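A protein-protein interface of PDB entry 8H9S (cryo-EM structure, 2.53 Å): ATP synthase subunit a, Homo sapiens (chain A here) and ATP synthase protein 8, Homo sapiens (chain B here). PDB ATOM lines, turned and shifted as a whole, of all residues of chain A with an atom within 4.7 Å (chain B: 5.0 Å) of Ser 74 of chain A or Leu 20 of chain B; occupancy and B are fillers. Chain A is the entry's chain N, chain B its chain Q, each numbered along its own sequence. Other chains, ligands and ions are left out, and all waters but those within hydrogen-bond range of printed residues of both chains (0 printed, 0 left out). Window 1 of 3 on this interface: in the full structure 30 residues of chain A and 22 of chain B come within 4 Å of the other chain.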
ATOM      1  N   SER A  69     -26.559 -33.249  23.783  1.00  0.00           N
ATOM      2  CA  SER A  69     -27.796 -33.176  23.017  1.00  0.00           C
ATOM      3  C   SER A  69     -28.165 -31.732  22.730  1.00  0.00           C
ATOM      4  O   SER A  69     -28.495 -31.379  21.594  1.00  0.00           O
ATOM      5  CB  SER A  69     -28.922 -33.877  23.766  1.00  0.00           C
ATOM      6  OG  SER A  69     -28.647 -35.253  23.911  1.00  0.00           O
ATOM      7  N   LEU A  70     -28.102 -30.882  23.753  1.00  0.00           N
ATOM      8  CA  LEU A  70     -28.401 -29.469  23.568  1.00  0.00           C
ATOM      9  C   LEU A  70     -27.484 -28.856  22.525  1.00  0.00           C
ATOM     10  O   LEU A  70     -27.938 -28.153  21.619  1.00  0.00           O
ATOM     11  CB  LEU A  70     -28.270 -28.734  24.897  1.00  0.00           C
ATOM     12  CG  LEU A  70     -28.900 -27.351  24.961  1.00  0.00           C
ATOM     13  CD1 LEU A  70     -30.382 -27.482  24.930  1.00  0.00           C
ATOM     14  CD2 LEU A  70     -28.474 -26.632  26.203  1.00  0.00           C
ATOM     15  N   MET A  71     -26.188 -29.150  22.617  1.00  0.00           N
ATOM     16  CA  MET A  71     -25.213 -28.536  21.726  1.00  0.00           C
ATOM     17  C   MET A  71     -25.423 -28.975  20.284  1.00  0.00           C
ATOM     18  O   MET A  71     -25.429 -28.145  19.371  1.00  0.00           O
ATOM     19  CB  MET A  71     -23.801 -28.872  22.194  1.00  0.00           C
ATOM     20  CG  MET A  71     -22.707 -28.339  21.304  1.00  0.00           C
ATOM     21  SD  MET A  71     -22.350 -26.608  21.599  1.00  0.00           S
ATOM     22  CE  MET A  71     -23.179 -25.860  20.209  1.00  0.00           C
ATOM     23  N   LEU A  72     -25.622 -30.270  20.055  1.00  0.00           N
ATOM     24  CA  LEU A  72     -25.720 -30.749  18.682  1.00  0.00           C
ATOM     25  C   LEU A  72     -27.066 -30.396  18.058  1.00  0.00           C
ATOM     26  O   LEU A  72     -27.131 -30.072  16.865  1.00  0.00           O
ATOM     27  CB  LEU A  72     -25.458 -32.249  18.633  1.00  0.00           C
ATOM     28  CG  LEU A  72     -24.017 -32.613  18.990  1.00  0.00           C
ATOM     29  CD1 LEU A  72     -23.697 -34.012  18.575  1.00  0.00           C
ATOM     30  CD2 LEU A  72     -23.037 -31.656  18.350  1.00  0.00           C
ATOM     31  N   VAL A  73     -28.146 -30.412  18.840  1.00  0.00           N
ATOM     32  CA  VAL A  73     -29.429 -29.989  18.295  1.00  0.00           C
ATOM     33  C   VAL A  73     -29.418 -28.495  18.002  1.00  0.00           C
ATOM     34  O   VAL A  73     -29.940 -28.050  16.976  1.00  0.00           O
ATOM     35  CB  VAL A  73     -30.572 -30.381  19.243  1.00  0.00           C
ATOM     36  CG1 VAL A  73     -31.879 -29.844  18.738  1.00  0.00           C
ATOM     37  CG2 VAL A  73     -30.648 -31.879  19.350  1.00  0.00           C
ATOM     38  N   SER A  74     -28.804 -27.696  18.877  1.00  0.00           N
ATOM     39  CA  SER A  74     -28.675 -26.275  18.593  1.00  0.00           C
ATOM     40  C   SER A  74     -27.849 -26.043  17.341  1.00  0.00           C
ATOM     41  O   SER A  74     -28.184 -25.186  16.519  1.00  0.00           O
ATOM     42  CB  SER A  74     -28.045 -25.569  19.783  1.00  0.00           C
ATOM     43  OG  SER A  74     -28.862 -25.707  20.923  1.00  0.00           O
ATOM     44  N   LEU A  75     -26.773 -26.810  17.170  1.00  0.00           N
ATOM     45  CA  LEU A  75     -25.931 -26.667  15.990  1.00  0.00           C
ATOM     46  C   LEU A  75     -26.714 -26.954  14.718  1.00  0.00           C
ATOM     47  O   LEU A  75     -26.673 -26.172  13.761  1.00  0.00           O
ATOM     48  CB  LEU A  75     -24.727 -27.595  16.110  1.00  0.00           C
ATOM     49  CG  LEU A  75     -23.625 -27.515  15.064  1.00  0.00           C
ATOM     50  CD1 LEU A  75     -22.944 -26.179  15.123  1.00  0.00           C
ATOM     51  CD2 LEU A  75     -22.639 -28.621  15.301  1.00  0.00           C
ATOM     52  N   ILE A  76     -27.449 -28.064  14.689  1.00  0.00           N
ATOM     53  CA  ILE A  76     -28.145 -28.420  13.457  1.00  0.00           C
ATOM     54  C   ILE A  76     -29.286 -27.449  13.177  1.00  0.00           C
ATOM     55  O   ILE A  76     -29.496 -27.048  12.028  1.00  0.00           O
ATOM     56  CB  ILE A  76     -28.625 -29.882  13.497  1.00  0.00           C
ATOM     57  CG1 ILE A  76     -29.213 -30.276  12.147  1.00  0.00           C
ATOM     58  CG2 ILE A  76     -29.639 -30.100  14.584  1.00  0.00           C
ATOM     59  CD1 ILE A  76     -29.240 -31.746  11.918  1.00  0.00           C
ATOM     60  N   ILE A  77     -30.013 -27.018  14.212  1.00  0.00           N
ATOM     61  CA  ILE A  77     -31.100 -26.063  14.003  1.00  0.00           C
ATOM     62  C   ILE A  77     -30.552 -24.741  13.482  1.00  0.00           C
ATOM     63  O   ILE A  77     -31.074 -24.167  12.519  1.00  0.00           O
ATOM     64  CB  ILE A  77     -31.899 -25.862  15.302  1.00  0.00           C
ATOM     65  CG1 ILE A  77     -32.573 -27.155  15.749  1.00  0.00           C
ATOM     66  CG2 ILE A  77     -32.934 -24.804  15.108  1.00  0.00           C
ATOM     67  CD1 ILE A  77     -33.789 -27.519  14.968  1.00  0.00           C
ATOM     68  N   PHE A  78     -29.484 -24.242  14.106  1.00  0.00           N
ATOM     69  CA  PHE A  78     -28.902 -22.965  13.717  1.00  0.00           C
ATOM     70  C   PHE A  78     -28.389 -23.007  12.285  1.00  0.00           C
ATOM     71  O   PHE A  78     -28.694 -22.119  11.480  1.00  0.00           O
ATOM     72  CB  PHE A  78     -27.787 -22.605  14.701  1.00  0.00           C
ATOM     73  CG  PHE A  78     -26.904 -21.482  14.253  1.00  0.00           C
ATOM     74  CD1 PHE A  78     -27.345 -20.179  14.286  1.00  0.00           C
ATOM     75  CD2 PHE A  78     -25.617 -21.730  13.830  1.00  0.00           C
ATOM     76  CE1 PHE A  78     -26.527 -19.154  13.882  1.00  0.00           C
ATOM     77  CE2 PHE A  78     -24.801 -20.706  13.428  1.00  0.00           C
ATOM     78  CZ  PHE A  78     -25.257 -19.419  13.454  1.00  0.00           C
ATOM     79  N   MET A 104     -17.154 -22.226  14.097  1.00  0.00           N
ATOM     80  CA  MET A 104     -18.041 -23.317  14.485  1.00  0.00           C
ATOM     81  C   MET A 104     -17.298 -24.644  14.548  1.00  0.00           C
ATOM     82  O   MET A 104     -17.589 -25.479  15.408  1.00  0.00           O
ATOM     83  CB  MET A 104     -19.208 -23.430  13.507  1.00  0.00           C
ATOM     84  CG  MET A 104     -20.322 -22.450  13.739  1.00  0.00           C
ATOM     85  SD  MET A 104     -21.845 -22.986  12.958  1.00  0.00           S
ATOM     86  CE  MET A 104     -21.357 -22.944  11.246  1.00  0.00           C
ATOM     87  N   PRO B  15     -21.249 -12.483  16.879  1.00  0.00           N
ATOM     88  CA  PRO B  15     -22.678 -12.801  17.023  1.00  0.00           C
ATOM     89  C   PRO B  15     -22.978 -14.283  16.926  1.00  0.00           C
ATOM     90  O   PRO B  15     -23.879 -14.766  17.621  1.00  0.00           O
ATOM     91  CB  PRO B  15     -23.331 -12.010  15.885  1.00  0.00           C
ATOM     92  CG  PRO B  15     -22.253 -11.702  14.961  1.00  0.00           C
ATOM     93  CD  PRO B  15     -21.034 -11.532  15.780  1.00  0.00           C
ATOM     94  N   MET B  16     -22.246 -15.024  16.094  1.00  0.00           N
ATOM     95  CA  MET B  16     -22.476 -16.461  15.991  1.00  0.00           C
ATOM     96  C   MET B  16     -22.334 -17.135  17.345  1.00  0.00           C
ATOM     97  O   MET B  16     -23.187 -17.933  17.745  1.00  0.00           O
ATOM     98  CB  MET B  16     -21.512 -17.082  14.986  1.00  0.00           C
ATOM     99  CG  MET B  16     -21.801 -18.535  14.683  1.00  0.00           C
ATOM    100  SD  MET B  16     -21.028 -19.689  15.825  1.00  0.00           S
ATOM    101  CE  MET B  16     -19.324 -19.205  15.662  1.00  0.00           C
ATOM    102  N   LEU B  17     -21.255 -16.829  18.069  1.00  0.00           N
ATOM    103  CA  LEU B  17     -21.055 -17.435  19.378  1.00  0.00           C
ATOM    104  C   LEU B  17     -22.185 -17.081  20.331  1.00  0.00           C
ATOM    105  O   LEU B  17     -22.477 -17.844  21.253  1.00  0.00           O
ATOM    106  CB  LEU B  17     -19.713 -17.003  19.966  1.00  0.00           C
ATOM    107  CG  LEU B  17     -18.452 -17.269  19.147  1.00  0.00           C
ATOM    108  CD1 LEU B  17     -17.331 -16.380  19.620  1.00  0.00           C
ATOM    109  CD2 LEU B  17     -18.042 -18.717  19.232  1.00  0.00           C
ATOM    110  N   LEU B  18     -22.834 -15.937  20.130  1.00  0.00           N
ATOM    111  CA  LEU B  18     -23.997 -15.623  20.947  1.00  0.00           C
ATOM    112  C   LEU B  18     -25.215 -16.400  20.481  1.00  0.00           C
ATOM    113  O   LEU B  18     -26.033 -16.828  21.298  1.00  0.00           O
ATOM    114  CB  LEU B  18     -24.285 -14.127  20.903  1.00  0.00           C
ATOM    115  CG  LEU B  18     -23.471 -13.276  21.863  1.00  0.00           C
ATOM    116  CD1 LEU B  18     -23.479 -11.836  21.411  1.00  0.00           C
ATOM    117  CD2 LEU B  18     -24.043 -13.402  23.253  1.00  0.00           C
ATOM    118  N   THR B  19     -25.347 -16.593  19.174  1.00  0.00           N
ATOM    119  CA  THR B  19     -26.522 -17.241  18.616  1.00  0.00           C
ATOM    120  C   THR B  19     -26.463 -18.752  18.760  1.00  0.00           C
ATOM    121  O   THR B  19     -27.494 -19.393  18.979  1.00  0.00           O
ATOM    122  CB  THR B  19     -26.652 -16.860  17.149  1.00  0.00           C
ATOM    123  OG1 THR B  19     -26.657 -15.438  17.036  1.00  0.00           O
ATOM    124  CG2 THR B  19     -27.912 -17.400  16.576  1.00  0.00           C
ATOM    125  N   LEU B  20     -25.278 -19.334  18.647  1.00  0.00           N
ATOM    126  CA  LEU B  20     -25.144 -20.780  18.692  1.00  0.00           C
ATOM    127  C   LEU B  20     -25.002 -21.305  20.109  1.00  0.00           C
ATOM    128  O   LEU B  20     -25.513 -22.383  20.418  1.00  0.00           O
ATOM    129  CB  LEU B  20     -23.942 -21.215  17.857  1.00  0.00           C
ATOM    130  CG  LEU B  20     -23.649 -22.707  17.851  1.00  0.00           C
ATOM    131  CD1 LEU B  20     -24.824 -23.446  17.289  1.00  0.00           C
ATOM    132  CD2 LEU B  20     -22.408 -22.989  17.048  1.00  0.00           C
ATOM    133  N   PHE B  21     -24.320 -20.567  20.981  1.00  0.00           N
ATOM    134  CA  PHE B  21     -24.026 -21.045  22.322  1.00  0.00           C
ATOM    135  C   PHE B  21     -24.906 -20.430  23.395  1.00  0.00           C
ATOM    136  O   PHE B  21     -24.888 -20.911  24.529  1.00  0.00           O
ATOM    137  CB  PHE B  21     -22.559 -20.780  22.672  1.00  0.00           C
ATOM    138  CG  PHE B  21     -21.598 -21.664  21.948  1.00  0.00           C
ATOM    139  CD1 PHE B  21     -21.333 -22.935  22.403  1.00  0.00           C
ATOM    140  CD2 PHE B  21     -20.965 -21.225  20.805  1.00  0.00           C
ATOM    141  CE1 PHE B  21     -20.451 -23.745  21.733  1.00  0.00           C
ATOM    142  CE2 PHE B  21     -20.085 -22.036  20.134  1.00  0.00           C
ATOM    143  CZ  PHE B  21     -19.829 -23.294  20.596  1.00  0.00           C
ATOM    144  N   LEU B  22     -25.654 -19.373  23.091  1.00  0.00           N
ATOM    145  CA  LEU B  22     -26.539 -18.782  24.085  1.00  0.00           C
ATOM    146  C   LEU B  22     -28.003 -18.811  23.674  1.00  0.00           C
ATOM    147  O   LEU B  22     -28.825 -19.349  24.414  1.00  0.00           O
ATOM    148  CB  LEU B  22     -26.096 -17.350  24.388  1.00  0.00           C
ATOM    149  CG  LEU B  22     -26.787 -16.699  25.577  1.00  0.00           C
ATOM    150  CD1 LEU B  22     -26.399 -17.419  26.840  1.00  0.00           C
ATOM    151  CD2 LEU B  22     -26.412 -15.243  25.659  1.00  0.00           C
ATOM    152  N   THR B  24     -29.873 -19.985  20.783  1.00  0.00           N
ATOM    153  CA  THR B  24     -30.481 -21.224  20.316  1.00  0.00           C
ATOM    154  C   THR B  24     -30.546 -22.254  21.430  1.00  0.00           C
ATOM    155  O   THR B  24     -31.504 -23.027  21.512  1.00  0.00           O
ATOM    156  CB  THR B  24     -29.707 -21.775  19.121  1.00  0.00           C
ATOM    157  OG1 THR B  24     -29.627 -20.773  18.107  1.00  0.00           O
ATOM    158  CG2 THR B  24     -30.413 -22.969  18.539  1.00  0.00           C
ATOM    159  N   GLN B  25     -29.560 -22.256  22.323  1.00  0.00           N
ATOM    160  CA  GLN B  25     -29.563 -23.218  23.413  1.00  0.00           C
ATOM    161  C   GLN B  25     -30.573 -22.841  24.485  1.00  0.00           C
ATOM    162  O   GLN B  25     -31.211 -23.716  25.075  1.00  0.00           O
ATOM    163  CB  GLN B  25     -28.162 -23.331  23.997  1.00  0.00           C
ATOM    164  CG  GLN B  25     -27.131 -23.662  22.952  1.00  0.00           C
ATOM    165  CD  GLN B  25     -25.979 -24.449  23.500  1.00  0.00           C
ATOM    166  OE1 GLN B  25     -26.018 -24.928  24.625  1.00  0.00           O
ATOM    167  NE2 GLN B  25     -24.941 -24.592  22.702  1.00  0.00           N
ATOM    168  N   MET B  28     -33.760 -24.090  23.027  1.00  0.00           N
ATOM    169  CA  MET B  28     -33.934 -25.533  23.124  1.00  0.00           C
ATOM    170  C   MET B  28     -34.218 -25.969  24.551  1.00  0.00           C
ATOM    171  O   MET B  28     -34.964 -26.927  24.761  1.00  0.00           O
ATOM    172  CB  MET B  28     -32.703 -26.269  22.604  1.00  0.00           C
ATOM    173  CG  MET B  28     -32.502 -26.178  21.116  1.00  0.00           C
ATOM    174  SD  MET B  28     -33.856 -26.900  20.197  1.00  0.00           S
ATOM    175  CE  MET B  28     -34.474 -25.449  19.362  1.00  0.00           C
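Printed residues of chain B within 4 Å of Leu 70 of chain A: Gln 25 (3.4 Å) and Met 28 (3.5 Å).
Of chain B, only Leu 20, Thr 24, Gln 25 and Met 28 come within 4 Å of Ser 74 of chain A.
Ile 77 of chain A touches none of the printed residues of chain B.
Leu 20 of chain B touches just these residues of chain A: Met 71, Ser 74, Leu 75, Phe 78 and Met 104.
Of the printed residues of chain A, Thr 24 of chain B touches Ser 74.
The nearest printed residue of chain B that does not touch Ser 74 of chain A is Thr 19 of chain B (6.3 Å).
The nearest printed residue of chain A that does not touch Leu 20 of chain B is Ile 76 of chain A (5.9 Å).
The nearest printed residue of chain A that does not touch Thr 24 of chain B is Phe 78 of chain A (4.3 Å).
Printed residues of chain B that touch a printed residue of chain A: Met 16, Thr 19, Leu 20, Phe 21, Thr 24, Gln 25 and Met 28.
Hydrophobic or aromatic side chains of chain B that line the printed part of chain A: Met 16, Leu 20, Phe 21 and Met 28.
Hydrophobic or aromatic side chains of chain A within 4 Å of the printed part of chain B: Leu 70, Met 71, Val 73, Leu 75, Phe 78 and Met 104.
Among the printed residues, no Asp or Glu carboxylate lies within 4 Å of a Lys or Arg side-chain nitrogen of the other chain.
The side-chain amide nitrogen (NE2) of Gln 25 of chain B lies within hydrogen-bond range of the backbone carbonyl oxygen (O) of Leu 20 of chain B, at 3.2 Å.
O of Leu 70 of chain A sits at hydrogen-bond distance from OG of Ser 74 of chain A (2.7 Å).
The backbone carbonyl oxygen of Thr 19 of chain B sits at hydrogen-bond distance from the side-chain hydroxyl of Thr 24 of chain B (2.7 Å).
O of Pro 15 of chain B is in hydrogen-bond range of OG1 of Thr 19 of chain B (2.9 Å).
Among the printed residues, pairs that only touch across the chains: Leu 70 of chain A with Gln 25 of chain B (3.4 Å), Leu 70 of chain A with Met 28 of chain B (3.5 Å), Met 71 of chain A with Leu 20 of chain B (3.97 Å), Met 71 of chain A with Phe 21 of chain B (3.4 Å), Val 73 of chain A with Met 28 of chain B (3.8 Å), Ser 74 of chain A with Leu 20 of chain B (3.9 Å), Ser 74 of chain A with Thr 24 of chain B (3.7 Å), Ser 74 of chain A with Gln 25 of chain B (3.4 Å), Ser 74 of chain A with Met 28 of chain B (3.7 Å), Leu 75 of chain A with Leu 20 of chain B (3.6 Å), Phe 78 of chain A with Met 16 of chain B (3.8 Å), Phe 78 of chain A with Thr 19 of chain B (3.5 Å), Phe 78 of chain A with Leu 20 of chain B (3.9 Å), Met 104 of chain A with Met 16 of chain B (3.5 Å) and Met 104 of chain A with Leu 20 of chain B (3.9 Å).
The side-chain sulfur (SD) of Met 71 of chain A sits close to the side-chain amide nitrogen (NE2) of Gln 25 of chain B (3.5 Å).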
